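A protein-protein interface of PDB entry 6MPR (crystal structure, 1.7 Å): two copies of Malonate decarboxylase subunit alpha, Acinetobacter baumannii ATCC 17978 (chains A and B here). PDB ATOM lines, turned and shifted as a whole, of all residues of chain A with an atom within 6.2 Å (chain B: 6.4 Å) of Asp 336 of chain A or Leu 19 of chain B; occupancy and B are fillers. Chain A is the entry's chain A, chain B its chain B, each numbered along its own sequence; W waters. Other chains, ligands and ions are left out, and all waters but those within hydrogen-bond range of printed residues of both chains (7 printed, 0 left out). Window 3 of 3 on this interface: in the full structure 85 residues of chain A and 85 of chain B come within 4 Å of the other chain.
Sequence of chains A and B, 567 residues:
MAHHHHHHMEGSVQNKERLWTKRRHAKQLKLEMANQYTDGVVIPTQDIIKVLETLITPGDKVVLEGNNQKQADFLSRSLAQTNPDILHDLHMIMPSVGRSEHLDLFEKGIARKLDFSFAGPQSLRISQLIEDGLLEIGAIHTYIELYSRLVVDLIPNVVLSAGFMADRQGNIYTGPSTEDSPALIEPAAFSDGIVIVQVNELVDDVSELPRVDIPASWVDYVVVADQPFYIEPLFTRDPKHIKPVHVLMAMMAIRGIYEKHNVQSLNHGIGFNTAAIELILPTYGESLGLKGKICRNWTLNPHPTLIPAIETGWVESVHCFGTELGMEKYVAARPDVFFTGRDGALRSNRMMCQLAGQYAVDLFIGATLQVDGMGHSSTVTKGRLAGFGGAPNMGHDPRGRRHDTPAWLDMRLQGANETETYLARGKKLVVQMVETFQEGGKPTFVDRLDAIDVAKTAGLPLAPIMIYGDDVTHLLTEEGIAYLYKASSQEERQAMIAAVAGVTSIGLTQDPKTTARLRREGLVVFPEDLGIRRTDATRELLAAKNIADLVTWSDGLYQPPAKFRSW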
ATOM      1  N   GLU A 316       3.207  30.094   4.085  1.00  0.00           N
ATOM      2  CA  GLU A 316       2.479  29.292   5.061  1.00  0.00           C
ATOM      3  C   GLU A 316       1.305  30.022   5.688  1.00  0.00           C
ATOM      4  O   GLU A 316       0.295  29.383   6.012  1.00  0.00           O
ATOM      5  CB  GLU A 316       3.443  28.799   6.143  1.00  0.00           C
ATOM      6  CG  GLU A 316       4.368  27.744   5.524  1.00  0.00           C
ATOM      7  CD  GLU A 316       5.481  27.269   6.430  1.00  0.00           C
ATOM      8  OE1 GLU A 316       6.423  26.644   5.896  1.00  0.00           O
ATOM      9  OE2 GLU A 316       5.423  27.511   7.657  1.00  0.00           O
ATOM     10  N   SER A 317       1.400  31.337   5.840  1.00  0.00           N
ATOM     11  CA  SER A 317       0.344  32.097   6.486  1.00  0.00           C
ATOM     12  C   SER A 317       0.405  33.536   5.999  1.00  0.00           C
ATOM     13  O   SER A 317       1.487  34.088   5.773  1.00  0.00           O
ATOM     14  CB  SER A 317       0.485  32.046   8.009  1.00  0.00           C
ATOM     15  OG  SER A 317       1.631  32.769   8.440  1.00  0.00           O
ATOM     16  N   ALA A 333     -10.716  30.050  -1.256  1.00  0.00           N
ATOM     17  CA  ALA A 333     -10.296  28.717  -1.635  1.00  0.00           C
ATOM     18  C   ALA A 333      -8.937  28.333  -1.062  1.00  0.00           C
ATOM     19  O   ALA A 333      -8.461  27.214  -1.336  1.00  0.00           O
ATOM     20  CB  ALA A 333     -10.281  28.588  -3.172  1.00  0.00           C
ATOM     21  N   ARG A 334      -8.319  29.213  -0.263  1.00  0.00           N
ATOM     22  CA  ARG A 334      -7.019  28.939   0.362  1.00  0.00           C
ATOM     23  C   ARG A 334      -7.052  29.173   1.877  1.00  0.00           C
ATOM     24  O   ARG A 334      -6.207  29.882   2.428  1.00  0.00           O
ATOM     25  CB  ARG A 334      -5.944  29.798  -0.298  1.00  0.00           C
ATOM     26  CG  ARG A 334      -5.785  29.555  -1.802  1.00  0.00           C
ATOM     27  CD  ARG A 334      -5.071  28.233  -2.060  1.00  0.00           C
ATOM     28  NE  ARG A 334      -4.864  27.945  -3.477  1.00  0.00           N
ATOM     29  CZ  ARG A 334      -5.788  27.412  -4.273  1.00  0.00           C
ATOM     30  NH1 ARG A 334      -6.997  27.115  -3.791  1.00  0.00           N
ATOM     31  NH2 ARG A 334      -5.503  27.158  -5.546  1.00  0.00           N
ATOM     32  N   PRO A 335      -8.019  28.581   2.589  1.00  0.00           N
ATOM     33  CA  PRO A 335      -8.172  28.917   4.012  1.00  0.00           C
ATOM     34  C   PRO A 335      -7.056  28.367   4.882  1.00  0.00           C
ATOM     35  O   PRO A 335      -6.910  28.834   6.014  1.00  0.00           O
ATOM     36  CB  PRO A 335      -9.520  28.298   4.376  1.00  0.00           C
ATOM     37  CG  PRO A 335      -9.647  27.137   3.458  1.00  0.00           C
ATOM     38  CD  PRO A 335      -9.020  27.591   2.156  1.00  0.00           C
ATOM     39  N   ASP A 336      -6.256  27.406   4.401  1.00  0.00           N
ATOM     40  CA  ASP A 336      -5.097  27.001   5.197  1.00  0.00           C
ATOM     41  C   ASP A 336      -4.069  28.120   5.342  1.00  0.00           C
ATOM     42  O   ASP A 336      -3.310  28.131   6.319  1.00  0.00           O
ATOM     43  CB  ASP A 336      -4.435  25.757   4.593  1.00  0.00           C
ATOM     44  CG  ASP A 336      -5.172  24.483   4.953  1.00  0.00           C
ATOM     45  OD1 ASP A 336      -5.978  24.536   5.903  1.00  0.00           O
ATOM     46  OD2 ASP A 336      -4.958  23.430   4.301  1.00  0.00           O
ATOM     47  N   VAL A 337      -4.044  29.063   4.409  1.00  0.00           N
ATOM     48  CA  VAL A 337      -3.049  30.126   4.372  1.00  0.00           C
ATOM     49  C   VAL A 337      -3.579  31.417   4.976  1.00  0.00           C
ATOM     50  O   VAL A 337      -2.891  32.058   5.766  1.00  0.00           O
ATOM     51  CB  VAL A 337      -2.574  30.346   2.920  1.00  0.00           C
ATOM     52  CG1 VAL A 337      -1.628  31.536   2.843  1.00  0.00           C
ATOM     53  CG2 VAL A 337      -1.892  29.067   2.434  1.00  0.00           C
ATOM     54  N   PHE A 338      -4.801  31.808   4.614  1.00  0.00           N
ATOM     55  CA  PHE A 338      -5.394  33.086   5.001  1.00  0.00           C
ATOM     56  C   PHE A 338      -6.275  32.934   6.239  1.00  0.00           C
ATOM     57  O   PHE A 338      -6.609  31.824   6.662  1.00  0.00           O
ATOM     58  CB  PHE A 338      -6.213  33.671   3.835  1.00  0.00           C
ATOM     59  CG  PHE A 338      -5.375  34.035   2.624  1.00  0.00           C
ATOM     60  CD1 PHE A 338      -4.722  35.256   2.565  1.00  0.00           C
ATOM     61  CD2 PHE A 338      -5.234  33.147   1.571  1.00  0.00           C
ATOM     62  CE1 PHE A 338      -3.938  35.601   1.478  1.00  0.00           C
ATOM     63  CE2 PHE A 338      -4.436  33.480   0.461  1.00  0.00           C
ATOM     64  CZ  PHE A 338      -3.789  34.712   0.423  1.00  0.00           C
ATOM     65  N   LEU B  19      -6.795  19.961  -0.418  1.00  0.00           N
ATOM     66  CA  LEU B  19      -5.415  20.133   0.016  1.00  0.00           C
ATOM     67  C   LEU B  19      -5.155  21.554   0.525  1.00  0.00           C
ATOM     68  O   LEU B  19      -4.044  21.863   0.957  1.00  0.00           O
ATOM     69  CB  LEU B  19      -4.438  19.777  -1.115  1.00  0.00           C
ATOM     70  CG  LEU B  19      -4.253  20.665  -2.352  1.00  0.00           C
ATOM     71  CD1 LEU B  19      -3.068  20.168  -3.168  1.00  0.00           C
ATOM     72  CD2 LEU B  19      -5.507  20.719  -3.215  1.00  0.00           C
ATOM     73  N   TRP B  20      -6.174  22.420   0.493  1.00  0.00           N
ATOM     74  CA  TRP B  20      -6.055  23.754   1.078  1.00  0.00           C
ATOM     75  C   TRP B  20      -7.037  23.974   2.218  1.00  0.00           C
ATOM     76  O   TRP B  20      -7.123  25.083   2.742  1.00  0.00           O
ATOM     77  CB  TRP B  20      -6.245  24.837   0.012  1.00  0.00           C
ATOM     78  CG  TRP B  20      -5.212  24.811  -1.078  1.00  0.00           C
ATOM     79  CD1 TRP B  20      -5.369  24.338  -2.345  1.00  0.00           C
ATOM     80  CD2 TRP B  20      -3.862  25.284  -0.989  1.00  0.00           C
ATOM     81  NE1 TRP B  20      -4.199  24.486  -3.061  1.00  0.00           N
ATOM     82  CE2 TRP B  20      -3.258  25.066  -2.248  1.00  0.00           C
ATOM     83  CE3 TRP B  20      -3.104  25.864   0.034  1.00  0.00           C
ATOM     84  CZ2 TRP B  20      -1.934  25.417  -2.515  1.00  0.00           C
ATOM     85  CZ3 TRP B  20      -1.784  26.220  -0.234  1.00  0.00           C
ATOM     86  CH2 TRP B  20      -1.217  25.996  -1.498  1.00  0.00           C
ATOM     87  N   THR B  21      -7.767  22.937   2.619  1.00  0.00           N
ATOM     88  CA  THR B  21      -8.772  22.989   3.671  1.00  0.00           C
ATOM     89  C   THR B  21      -8.425  22.042   4.818  1.00  0.00           C
ATOM     90  O   THR B  21      -9.318  21.509   5.488  1.00  0.00           O
ATOM     91  CB  THR B  21     -10.137  22.625   3.099  1.00  0.00           C
ATOM     92  OG1 THR B  21     -10.047  21.317   2.516  1.00  0.00           O
ATOM     93  CG2 THR B  21     -10.518  23.611   2.017  1.00  0.00           C
ATOM     94  N   LYS B  22      -7.129  21.811   5.045  1.00  0.00           N
ATOM     95  CA  LYS B  22      -6.713  20.867   6.080  1.00  0.00           C
ATOM     96  C   LYS B  22      -7.128  21.329   7.478  1.00  0.00           C
ATOM     97  O   LYS B  22      -7.593  20.519   8.291  1.00  0.00           O
ATOM     98  CB  LYS B  22      -5.202  20.660   6.018  1.00  0.00           C
ATOM     99  CG  LYS B  22      -4.714  19.927   4.767  1.00  0.00           C
ATOM    100  CD  LYS B  22      -3.228  19.635   4.871  1.00  0.00           C
ATOM    101  CE  LYS B  22      -2.715  18.898   3.648  1.00  0.00           C
ATOM    102  NZ  LYS B  22      -2.492  19.832   2.506  1.00  0.00           N
ATOM    103  N   ARG B  23      -6.947  22.615   7.791  1.00  0.00           N
ATOM    104  CA  ARG B  23      -7.338  23.091   9.114  1.00  0.00           C
ATOM    105  C   ARG B  23      -8.840  22.948   9.299  1.00  0.00           C
ATOM    106  O   ARG B  23      -9.309  22.450  10.328  1.00  0.00           O
ATOM    107  CB  ARG B  23      -6.907  24.549   9.306  1.00  0.00           C
ATOM    108  CG  ARG B  23      -5.396  24.737   9.276  1.00  0.00           C
ATOM    109  CD  ARG B  23      -4.967  26.100   9.817  1.00  0.00           C
ATOM    110  NE  ARG B  23      -5.518  27.224   9.053  1.00  0.00           N
ATOM    111  CZ  ARG B  23      -5.018  28.456   9.095  1.00  0.00           C
ATOM    112  NH1 ARG B  23      -3.957  28.714   9.851  1.00  0.00           N
ATOM    113  NH2 ARG B  23      -5.571  29.433   8.387  1.00  0.00           N
ATOM    114  N   ARG B  24      -9.605  23.399   8.300  1.00  0.00           N
ATOM    115  CA  ARG B  24     -11.059  23.301   8.354  1.00  0.00           C
ATOM    116  C   ARG B  24     -11.501  21.868   8.593  1.00  0.00           C
ATOM    117  O   ARG B  24     -12.324  21.596   9.471  1.00  0.00           O
ATOM    118  CB  ARG B  24     -11.665  23.824   7.049  1.00  0.00           C
ATOM    119  CG  ARG B  24     -13.185  23.567   6.924  1.00  0.00           C
ATOM    120  CD  ARG B  24     -13.724  24.163   5.623  1.00  0.00           C
ATOM    121  NE  ARG B  24     -13.531  25.614   5.625  1.00  0.00           N
ATOM    122  CZ  ARG B  24     -13.482  26.373   4.533  1.00  0.00           C
ATOM    123  NH1 ARG B  24     -13.597  25.817   3.329  1.00  0.00           N
ATOM    124  NH2 ARG B  24     -13.289  27.685   4.656  1.00  0.00           N
ATOM    125  N   ASP B 192      -9.643  28.407  11.886  1.00  0.00           N
ATOM    126  CA  ASP B 192     -10.139  27.086  12.267  1.00  0.00           C
ATOM    127  C   ASP B 192      -9.431  26.570  13.515  1.00  0.00           C
ATOM    128  O   ASP B 192      -9.170  25.372  13.653  1.00  0.00           O
ATOM    129  CB  ASP B 192     -10.052  26.094  11.093  1.00  0.00           C
ATOM    130  CG  ASP B 192     -11.091  26.391  10.016  1.00  0.00           C
ATOM    131  OD1 ASP B 192     -12.292  26.091  10.227  1.00  0.00           O
ATOM    132  OD2 ASP B 192     -10.720  26.960   8.964  1.00  0.00           O
HETATM  133  O   HOH W   1      -8.720  30.264   7.679  1.00  0.00           O
HETATM  134  O   HOH W   2      -3.630  31.572   8.798  1.00  0.00           O
HETATM  135  O   HOH W   3      -1.569  29.462   8.013  1.00  0.00           O
HETATM  136  O   HOH W   4      -2.432  23.277   3.109  1.00  0.00           O
HETATM  137  O   HOH W   5      -3.163  24.627  -5.930  1.00  0.00           O
HETATM  138  O   HOH W   6      -8.420  27.486   7.966  1.00  0.00           O
HETATM  139  O   HOH W   7      -8.605  25.342   6.207  1.00  0.00           O
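Water W6 lies within hydrogen-bond range of the side-chain carboxylate of Asp 192 of chain B, the backbone carbonyl oxygen of Pro 335 of chain A and the guanidinium group of Arg 23 of chain B. Water W3 lies within hydrogen-bond range of O of Glu 316 of chain A (2.7 Å), O of Asp 336 of chain A (2.8 Å) and NH1 of Arg 23 of chain B (3.1 Å). Water W7 lies within hydrogen-bond range of OD1 of Asp 336 of chain A (2.8 Å) and N of Arg 24 of chain B (3.0 Å). Water W4 lies within hydrogen-bond range of the side-chain carboxylate of Asp 336 of chain A, the backbone carbonyl oxygen of Leu 19 of chain B and the side-chain amino group of Lys 22 of chain B. Water W1 lies within hydrogen-bond range of the backbone carbonyl oxygen (O) of Phe 338 of chain A, the backbone carbonyl oxygen (O) of Pro 335 of chain A and the guanidinium group (NH2) of Arg 23 of chain B. Water W2 bridges the guanidinium group of Arg 23 of chain B and the backbone carbonyl oxygen of Val 337 of chain A.
Ala 333 of chain A touches Trp 20 of chain B (O to CB, 3.5 Å). Arg 334 of chain A touches Trp 20 of chain B. Trp 20 of chain B touches Pro 335 of chain A (O to CD, 3.2 Å). Pro 335 of chain A touches Thr 21 of chain B. Pro 335 of chain A touches Arg 24 of chain B. OD2 of Asp 336 of chain A touches O of Leu 19 of chain B, at 3.8 Å. Val 337 of chain A touches Trp 20 of chain B (CG2 to CZ3, 3.9 Å).
NH2 of Arg 23 of chain B sits at hydrogen-bond distance from O of Pro 335 of chain A, at 2.8 Å. The backbone NH of Asp 336 of chain A sits at hydrogen-bond distance from the backbone carbonyl oxygen of Trp 20 of chain B, 3.0 Å away. The side-chain carboxylate (OD2) of Asp 336 of chain A is in hydrogen-bond range of the backbone NH (N) of Thr 21 of chain B, at 3.3 Å. The side-chain carboxylate (OD2) of Asp 336 of chain A sits at hydrogen-bond distance from the backbone NH (N) of Lys 22 of chain B, at 2.8 Å. The side-chain carboxylate (OD1) of Asp 336 of chain A lies within hydrogen-bond range of the backbone NH (N) of Arg 23 of chain B, at 2.9 Å. O of Phe 338 of chain A sits at hydrogen-bond distance from NH2 of Arg 23 of chain B (3.1 Å).
Leu 19 of chain B touches just one residue of chain A: Asp 336 (3.8 Å). Of the printed residues of chain A, Thr 21 of chain B touches Pro 335 and Asp 336. Printed residues of chain B within 4 Å of Arg 334 of chain A: Trp 20 (3.4 Å). Printed residues of chain A within 4 Å of Trp 20 of chain B: Ala 333, Arg 334, Pro 335, Asp 336 and Val 337. Of the printed residues of chain B, Pro 335 of chain A touches Trp 20 (3.2 Å), Thr 21 (3.9 Å), Arg 23 (2.8 Å) and Arg 24 (3.8 Å). Asp 192 of chain B touches none of the printed residues of chain A.
Among the printed residues, no Asp or Glu carboxylate lies within 4 Å of a Lys or Arg side-chain nitrogen of the other chain.
No position is printed for both chains.
The backbone carbonyl oxygen (O) of Leu 19 of chain B is in hydrogen-bond range of the side-chain amino group (NZ) of Lys 22 of chain B (3.0 Å).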
